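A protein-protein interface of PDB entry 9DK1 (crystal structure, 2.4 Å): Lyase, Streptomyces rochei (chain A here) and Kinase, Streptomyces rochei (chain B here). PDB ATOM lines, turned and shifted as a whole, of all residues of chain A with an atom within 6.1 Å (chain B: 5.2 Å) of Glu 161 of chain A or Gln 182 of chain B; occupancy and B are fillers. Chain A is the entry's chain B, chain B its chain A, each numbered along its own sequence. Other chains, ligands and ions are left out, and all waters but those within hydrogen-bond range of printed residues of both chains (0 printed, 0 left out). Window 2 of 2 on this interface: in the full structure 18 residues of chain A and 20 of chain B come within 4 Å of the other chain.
O of Glu 161 of chain A sits at hydrogen-bond distance from NH2 of Arg 164 of chain A (2.7 Å).
The backbone NH of Thr 109 of chain A lies within hydrogen-bond range of the backbone carbonyl oxygen of Leu 160 of chain A (2.9 Å).
OE2 of Glu 161 of chain A lies within salt-bridge range of NH2 of Arg 142 of chain A (2.6 Å).
NE1 of Trp 178 of chain B sits close to OE1 of Gln 182 of chain B (3.0 Å).
The guanidinium group (NH1) of Arg 184 of chain B sits close to the backbone carbonyl oxygen (O) of Ala 180 of chain B.
The side-chain carboxylate (OE1) of Glu 161 of chain A lies within hydrogen-bond range of the indole nitrogen (NE1) of Trp 178 of chain B (2.7 Å).
The side-chain amide nitrogen of Gln 182 of chain B lies within hydrogen-bond range of the side-chain carboxylate of Glu 161 of chain A (3.3 Å).
Among the printed residues, merely in contact across the chains: Ala 166 of chain A with Arg 184 of chain B (3.6 Å), Leu 167 of chain A with Arg 184 of chain B (3.6 Å), Ala 166 of chain A with Glu 183 of chain B (3.6 Å), Arg 164 of chain A with Trp 178 of chain B (3.6 Å) and Leu 160 of chain A with Trp 178 of chain B (3.7 Å).
Hydrophobic or aromatic side chains of chain A within 4 Å of the printed part of chain B: Leu 160 and Ala 166.
Hydrophobic or aromatic side chains of chain B within 4 Å of the printed part of chain A: Trp 178.
Among the printed residues, 7 pairs touch across the chains.
Arg 92 of chain A touches none of the printed residues of chain B.
Printed residues of chain B within 4 Å of Leu 160 of chain A: Trp 178.
Of chain B, only Trp 178 (2.7 Å) and Gln 182 (3.3 Å) come within 4 Å of Glu 161 of chain A.
Of the printed residues of chain B, Arg 164 of chain A touches Trp 178 (3.6 Å).
Ala 180 of chain B touches none of the printed residues of chain A.
Gln 182 of chain B touches just one residue of chain A: Glu 161 (3.3 Å).
Printed residues of chain A within 4 Å of Arg 184 of chain B: Ala 166 (3.6 Å) and Leu 167 (3.6 Å).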
ATOM      1  N   ARG A  92     -27.836 -27.887  12.650  1.00  0.00           N
ATOM      2  CA  ARG A  92     -28.375 -27.682  11.307  1.00  0.00           C
ATOM      3  C   ARG A  92     -27.970 -28.842  10.395  1.00  0.00           C
ATOM      4  O   ARG A  92     -26.806 -29.230  10.340  1.00  0.00           O
ATOM      5  CB  ARG A  92     -27.857 -26.370  10.696  1.00  0.00           C
ATOM      6  CG  ARG A  92     -28.502 -25.095  11.233  1.00  0.00           C
ATOM      7  CD  ARG A  92     -27.689 -23.822  11.004  1.00  0.00           C
ATOM      8  NE  ARG A  92     -27.348 -23.558   9.605  1.00  0.00           N
ATOM      9  CZ  ARG A  92     -26.633 -22.517   9.172  1.00  0.00           C
ATOM     10  NH1 ARG A  92     -25.868 -21.831  10.002  1.00  0.00           N
ATOM     11  NH2 ARG A  92     -26.676 -22.163   7.901  1.00  0.00           N
ATOM     12  N   ARG A 107     -37.079 -15.850  -3.677  1.00  0.00           N
ATOM     13  CA  ARG A 107     -35.663 -15.813  -3.300  1.00  0.00           C
ATOM     14  C   ARG A 107     -35.278 -14.507  -2.597  1.00  0.00           C
ATOM     15  O   ARG A 107     -34.242 -14.452  -1.951  1.00  0.00           O
ATOM     16  CB  ARG A 107     -34.766 -15.987  -4.535  1.00  0.00           C
ATOM     17  CG  ARG A 107     -34.773 -17.388  -5.146  1.00  0.00           C
ATOM     18  CD  ARG A 107     -34.224 -18.471  -4.235  1.00  0.00           C
ATOM     19  NE  ARG A 107     -34.287 -19.824  -4.787  1.00  0.00           N
ATOM     20  CZ  ARG A 107     -34.535 -20.934  -4.087  1.00  0.00           C
ATOM     21  NH1 ARG A 107     -35.771 -21.282  -3.767  1.00  0.00           N
ATOM     22  NH2 ARG A 107     -33.533 -21.753  -3.816  1.00  0.00           N
ATOM     23  N   THR A 108     -36.115 -13.474  -2.708  1.00  0.00           N
ATOM     24  CA  THR A 108     -35.729 -12.106  -2.426  1.00  0.00           C
ATOM     25  C   THR A 108     -36.879 -11.404  -1.725  1.00  0.00           C
ATOM     26  O   THR A 108     -38.033 -11.653  -2.047  1.00  0.00           O
ATOM     27  CB  THR A 108     -35.326 -11.357  -3.703  1.00  0.00           C
ATOM     28  OG1 THR A 108     -34.213 -12.108  -4.182  1.00  0.00           O
ATOM     29  CG2 THR A 108     -34.905  -9.911  -3.516  1.00  0.00           C
ATOM     30  N   THR A 109     -36.505 -10.552  -0.755  1.00  0.00           N
ATOM     31  CA  THR A 109     -37.405  -9.708  -0.001  1.00  0.00           C
ATOM     32  C   THR A 109     -36.869  -8.288  -0.061  1.00  0.00           C
ATOM     33  O   THR A 109     -35.777  -8.025   0.434  1.00  0.00           O
ATOM     34  CB  THR A 109     -37.485 -10.107   1.480  1.00  0.00           C
ATOM     35  OG1 THR A 109     -37.657 -11.519   1.592  1.00  0.00           O
ATOM     36  CG2 THR A 109     -38.611  -9.371   2.168  1.00  0.00           C
ATOM     37  N   ARG A 142     -27.642  -4.515  -5.157  1.00  0.00           N
ATOM     38  CA  ARG A 142     -28.876  -5.027  -4.524  1.00  0.00           C
ATOM     39  C   ARG A 142     -29.853  -3.861  -4.371  1.00  0.00           C
ATOM     40  O   ARG A 142     -30.990  -4.096  -3.960  1.00  0.00           O
ATOM     41  CB  ARG A 142     -28.517  -5.734  -3.218  1.00  0.00           C
ATOM     42  CG  ARG A 142     -28.110  -7.187  -3.409  1.00  0.00           C
ATOM     43  CD  ARG A 142     -26.964  -7.566  -2.501  1.00  0.00           C
ATOM     44  NE  ARG A 142     -26.589  -8.965  -2.619  1.00  0.00           N
ATOM     45  CZ  ARG A 142     -27.321  -9.984  -2.191  1.00  0.00           C
ATOM     46  NH1 ARG A 142     -28.491  -9.766  -1.618  1.00  0.00           N
ATOM     47  NH2 ARG A 142     -26.881 -11.217  -2.343  1.00  0.00           N
ATOM     48  N   ALA A 159     -32.701  -5.708  -2.400  1.00  0.00           N
ATOM     49  CA  ALA A 159     -32.996  -7.100  -2.633  1.00  0.00           C
ATOM     50  C   ALA A 159     -32.141  -7.920  -1.688  1.00  0.00           C
ATOM     51  O   ALA A 159     -30.978  -8.235  -1.993  1.00  0.00           O
ATOM     52  CB  ALA A 159     -32.702  -7.447  -4.070  1.00  0.00           C
ATOM     53  N   LEU A 160     -32.718  -8.213  -0.531  1.00  0.00           N
ATOM     54  CA  LEU A 160     -31.999  -9.013   0.475  1.00  0.00           C
ATOM     55  C   LEU A 160     -32.586 -10.414   0.428  1.00  0.00           C
ATOM     56  O   LEU A 160     -33.788 -10.538   0.221  1.00  0.00           O
ATOM     57  CB  LEU A 160     -32.160  -8.334   1.834  1.00  0.00           C
ATOM     58  CG  LEU A 160     -31.438  -6.998   1.987  1.00  0.00           C
ATOM     59  CD1 LEU A 160     -31.433  -6.548   3.436  1.00  0.00           C
ATOM     60  CD2 LEU A 160     -30.018  -7.084   1.454  1.00  0.00           C
ATOM     61  N   GLU A 161     -31.744 -11.415   0.601  1.00  0.00           N
ATOM     62  CA  GLU A 161     -32.185 -12.823   0.555  1.00  0.00           C
ATOM     63  C   GLU A 161     -33.352 -13.048   1.504  1.00  0.00           C
ATOM     64  O   GLU A 161     -33.370 -12.434   2.563  1.00  0.00           O
ATOM     65  CB  GLU A 161     -31.019 -13.747   0.894  1.00  0.00           C
ATOM     66  CG  GLU A 161     -30.040 -13.933  -0.248  1.00  0.00           C
ATOM     67  CD  GLU A 161     -28.891 -12.943  -0.265  1.00  0.00           C
ATOM     68  OE1 GLU A 161     -28.953 -11.959   0.484  1.00  0.00           O
ATOM     69  OE2 GLU A 161     -27.945 -13.162  -1.031  1.00  0.00           O
ATOM     70  N   ALA A 162     -34.271 -13.921   1.107  1.00  0.00           N
ATOM     71  CA  ALA A 162     -35.454 -14.248   1.923  1.00  0.00           C
ATOM     72  C   ALA A 162     -35.133 -15.408   2.863  1.00  0.00           C
ATOM     73  O   ALA A 162     -35.685 -15.433   3.953  1.00  0.00           O
ATOM     74  CB  ALA A 162     -36.581 -14.580   0.995  1.00  0.00           C
ATOM     75  N   ALA A 163     -34.250 -16.313   2.447  1.00  0.00           N
ATOM     76  CA  ALA A 163     -33.864 -17.394   3.337  1.00  0.00           C
ATOM     77  C   ALA A 163     -32.830 -16.889   4.342  1.00  0.00           C
ATOM     78  O   ALA A 163     -31.872 -16.247   3.954  1.00  0.00           O
ATOM     79  CB  ALA A 163     -33.317 -18.558   2.570  1.00  0.00           C
ATOM     80  N   ARG A 164     -33.074 -17.190   5.628  1.00  0.00           N
ATOM     81  CA  ARG A 164     -32.198 -16.887   6.742  1.00  0.00           C
ATOM     82  C   ARG A 164     -32.039 -18.160   7.585  1.00  0.00           C
ATOM     83  O   ARG A 164     -32.778 -18.402   8.536  1.00  0.00           O
ATOM     84  CB  ARG A 164     -32.777 -15.703   7.516  1.00  0.00           C
ATOM     85  CG  ARG A 164     -33.023 -14.453   6.683  1.00  0.00           C
ATOM     86  CD  ARG A 164     -31.754 -13.811   6.151  1.00  0.00           C
ATOM     87  NE  ARG A 164     -32.046 -12.730   5.215  1.00  0.00           N
ATOM     88  CZ  ARG A 164     -32.529 -11.540   5.556  1.00  0.00           C
ATOM     89  NH1 ARG A 164     -32.428 -11.099   6.804  1.00  0.00           N
ATOM     90  NH2 ARG A 164     -33.102 -10.787   4.633  1.00  0.00           N
ATOM     91  N   PRO A 165     -31.114 -19.071   7.214  1.00  0.00           N
ATOM     92  CA  PRO A 165     -30.918 -20.340   7.938  1.00  0.00           C
ATOM     93  C   PRO A 165     -30.265 -20.358   9.319  1.00  0.00           C
ATOM     94  O   PRO A 165     -30.374 -21.354  10.044  1.00  0.00           O
ATOM     95  CB  PRO A 165     -30.034 -21.176   6.988  1.00  0.00           C
ATOM     96  CG  PRO A 165     -29.431 -20.185   6.007  1.00  0.00           C
ATOM     97  CD  PRO A 165     -30.377 -19.012   5.938  1.00  0.00           C
ATOM     98  N   ALA A 166     -29.620 -19.250   9.688  1.00  0.00           N
ATOM     99  CA  ALA A 166     -28.952 -19.089  10.976  1.00  0.00           C
ATOM    100  C   ALA A 166     -29.754 -18.194  11.916  1.00  0.00           C
ATOM    101  O   ALA A 166     -29.501 -18.193  13.106  1.00  0.00           O
ATOM    102  CB  ALA A 166     -27.564 -18.500  10.771  1.00  0.00           C
ATOM    103  N   LEU A 167     -30.727 -17.441  11.389  1.00  0.00           N
ATOM    104  CA  LEU A 167     -31.375 -16.388  12.151  1.00  0.00           C
ATOM    105  C   LEU A 167     -31.981 -16.934  13.447  1.00  0.00           C
ATOM    106  O   LEU A 167     -31.800 -16.375  14.530  1.00  0.00           O
ATOM    107  CB  LEU A 167     -32.426 -15.720  11.266  1.00  0.00           C
ATOM    108  CG  LEU A 167     -33.134 -14.525  11.917  1.00  0.00           C
ATOM    109  CD1 LEU A 167     -32.141 -13.462  12.342  1.00  0.00           C
ATOM    110  CD2 LEU A 167     -34.188 -13.916  10.986  1.00  0.00           C
ATOM    111  N   MET A 175     -38.334 -14.987   5.055  1.00  0.00           N
ATOM    112  CA  MET A 175     -39.214 -13.823   5.033  1.00  0.00           C
ATOM    113  C   MET A 175     -39.942 -13.931   3.697  1.00  0.00           C
ATOM    114  O   MET A 175     -39.342 -14.426   2.750  1.00  0.00           O
ATOM    115  CB  MET A 175     -38.369 -12.556   5.092  1.00  0.00           C
ATOM    116  CG  MET A 175     -37.160 -12.697   5.979  1.00  0.00           C
ATOM    117  SD  MET A 175     -36.516 -11.096   6.476  1.00  0.00           S
ATOM    118  CE  MET A 175     -35.858 -11.499   8.091  1.00  0.00           C
ATOM    119  N   TRP B 178     -22.904  -7.961   4.774  1.00  0.00           N
ATOM    120  CA  TRP B 178     -24.197  -8.593   4.584  1.00  0.00           C
ATOM    121  C   TRP B 178     -24.077 -10.112   4.713  1.00  0.00           C
ATOM    122  O   TRP B 178     -24.951 -10.769   5.266  1.00  0.00           O
ATOM    123  CB  TRP B 178     -24.849  -8.199   3.254  1.00  0.00           C
ATOM    124  CG  TRP B 178     -26.148  -8.919   3.073  1.00  0.00           C
ATOM    125  CD1 TRP B 178     -26.460  -9.817   2.099  1.00  0.00           C
ATOM    126  CD2 TRP B 178     -27.284  -8.876   3.964  1.00  0.00           C
ATOM    127  NE1 TRP B 178     -27.727 -10.309   2.303  1.00  0.00           N
ATOM    128  CE2 TRP B 178     -28.251  -9.765   3.444  1.00  0.00           C
ATOM    129  CE3 TRP B 178     -27.571  -8.192   5.154  1.00  0.00           C
ATOM    130  CZ2 TRP B 178     -29.481  -9.978   4.064  1.00  0.00           C
ATOM    131  CZ3 TRP B 178     -28.778  -8.410   5.776  1.00  0.00           C
ATOM    132  CH2 TRP B 178     -29.720  -9.288   5.232  1.00  0.00           C
ATOM    133  N   SER B 179     -22.988 -10.691   4.209  1.00  0.00           N
ATOM    134  CA  SER B 179     -22.845 -12.143   4.214  1.00  0.00           C
ATOM    135  C   SER B 179     -22.645 -12.685   5.636  1.00  0.00           C
ATOM    136  O   SER B 179     -22.881 -13.857   5.885  1.00  0.00           O
ATOM    137  CB  SER B 179     -21.727 -12.543   3.264  1.00  0.00           C
ATOM    138  OG  SER B 179     -20.507 -11.880   3.606  1.00  0.00           O
ATOM    139  N   ALA B 180     -22.172 -11.842   6.559  1.00  0.00           N
ATOM    140  CA  ALA B 180     -21.981 -12.192   7.955  1.00  0.00           C
ATOM    141  C   ALA B 180     -23.303 -12.073   8.718  1.00  0.00           C
ATOM    142  O   ALA B 180     -23.569 -12.820   9.654  1.00  0.00           O
ATOM    143  CB  ALA B 180     -20.962 -11.271   8.572  1.00  0.00           C
ATOM    144  N   VAL B 181     -24.134 -11.112   8.335  1.00  0.00           N
ATOM    145  CA  VAL B 181     -25.481 -11.052   8.864  1.00  0.00           C
ATOM    146  C   VAL B 181     -26.231 -12.353   8.547  1.00  0.00           C
ATOM    147  O   VAL B 181     -27.021 -12.828   9.359  1.00  0.00           O
ATOM    148  CB  VAL B 181     -26.247  -9.839   8.312  1.00  0.00           C
ATOM    149  CG1 VAL B 181     -27.702  -9.881   8.738  1.00  0.00           C
ATOM    150  CG2 VAL B 181     -25.611  -8.531   8.727  1.00  0.00           C
ATOM    151  N   GLN B 182     -26.003 -12.929   7.388  1.00  0.00           N
ATOM    152  CA  GLN B 182     -26.800 -14.110   6.987  1.00  0.00           C
ATOM    153  C   GLN B 182     -26.231 -15.383   7.604  1.00  0.00           C
ATOM    154  O   GLN B 182     -26.735 -16.437   7.315  1.00  0.00           O
ATOM    155  CB  GLN B 182     -26.893 -14.198   5.465  1.00  0.00           C
ATOM    156  CG  GLN B 182     -27.083 -12.885   4.736  1.00  0.00           C
ATOM    157  CD  GLN B 182     -26.812 -13.123   3.274  1.00  0.00           C
ATOM    158  OE1 GLN B 182     -25.877 -12.583   2.696  1.00  0.00           O
ATOM    159  NE2 GLN B 182     -27.617 -13.978   2.671  1.00  0.00           N
ATOM    160  N   GLU B 183     -25.236 -15.255   8.468  1.00  0.00           N
ATOM    161  CA  GLU B 183     -24.641 -16.435   9.138  1.00  0.00           C
ATOM    162  C   GLU B 183     -24.736 -16.269  10.652  1.00  0.00           C
ATOM    163  O   GLU B 183     -24.075 -17.022  11.358  1.00  0.00           O
ATOM    164  CB  GLU B 183     -23.184 -16.623   8.724  1.00  0.00           C
ATOM    165  CG  GLU B 183     -22.956 -16.792   7.239  1.00  0.00           C
ATOM    166  CD  GLU B 183     -21.483 -16.771   6.867  1.00  0.00           C
ATOM    167  OE1 GLU B 183     -20.728 -15.999   7.492  1.00  0.00           O
ATOM    168  OE2 GLU B 183     -21.092 -17.528   5.960  1.00  0.00           O
ATOM    169  N   ARG B 184     -25.568 -15.349  11.119  1.00  0.00           N
ATOM    170  CA  ARG B 184     -25.678 -15.090  12.540  1.00  0.00           C
ATOM    171  C   ARG B 184     -27.126 -15.215  13.002  1.00  0.00           C
ATOM    172  O   ARG B 184     -28.061 -15.046  12.219  1.00  0.00           O
ATOM    173  CB  ARG B 184     -25.298 -13.648  12.868  1.00  0.00           C
ATOM    174  CG  ARG B 184     -23.880 -13.274  12.501  1.00  0.00           C
ATOM    175  CD  ARG B 184     -22.902 -13.928  13.426  1.00  0.00           C
ATOM    176  NE  ARG B 184     -21.575 -13.401  13.168  1.00  0.00           N
ATOM    177  CZ  ARG B 184     -20.811 -13.781  12.162  1.00  0.00           C
ATOM    178  NH1 ARG B 184     -21.355 -14.209  11.035  1.00  0.00           N
ATOM    179  NH2 ARG B 184     -19.505 -13.717  12.301  1.00  0.00           N
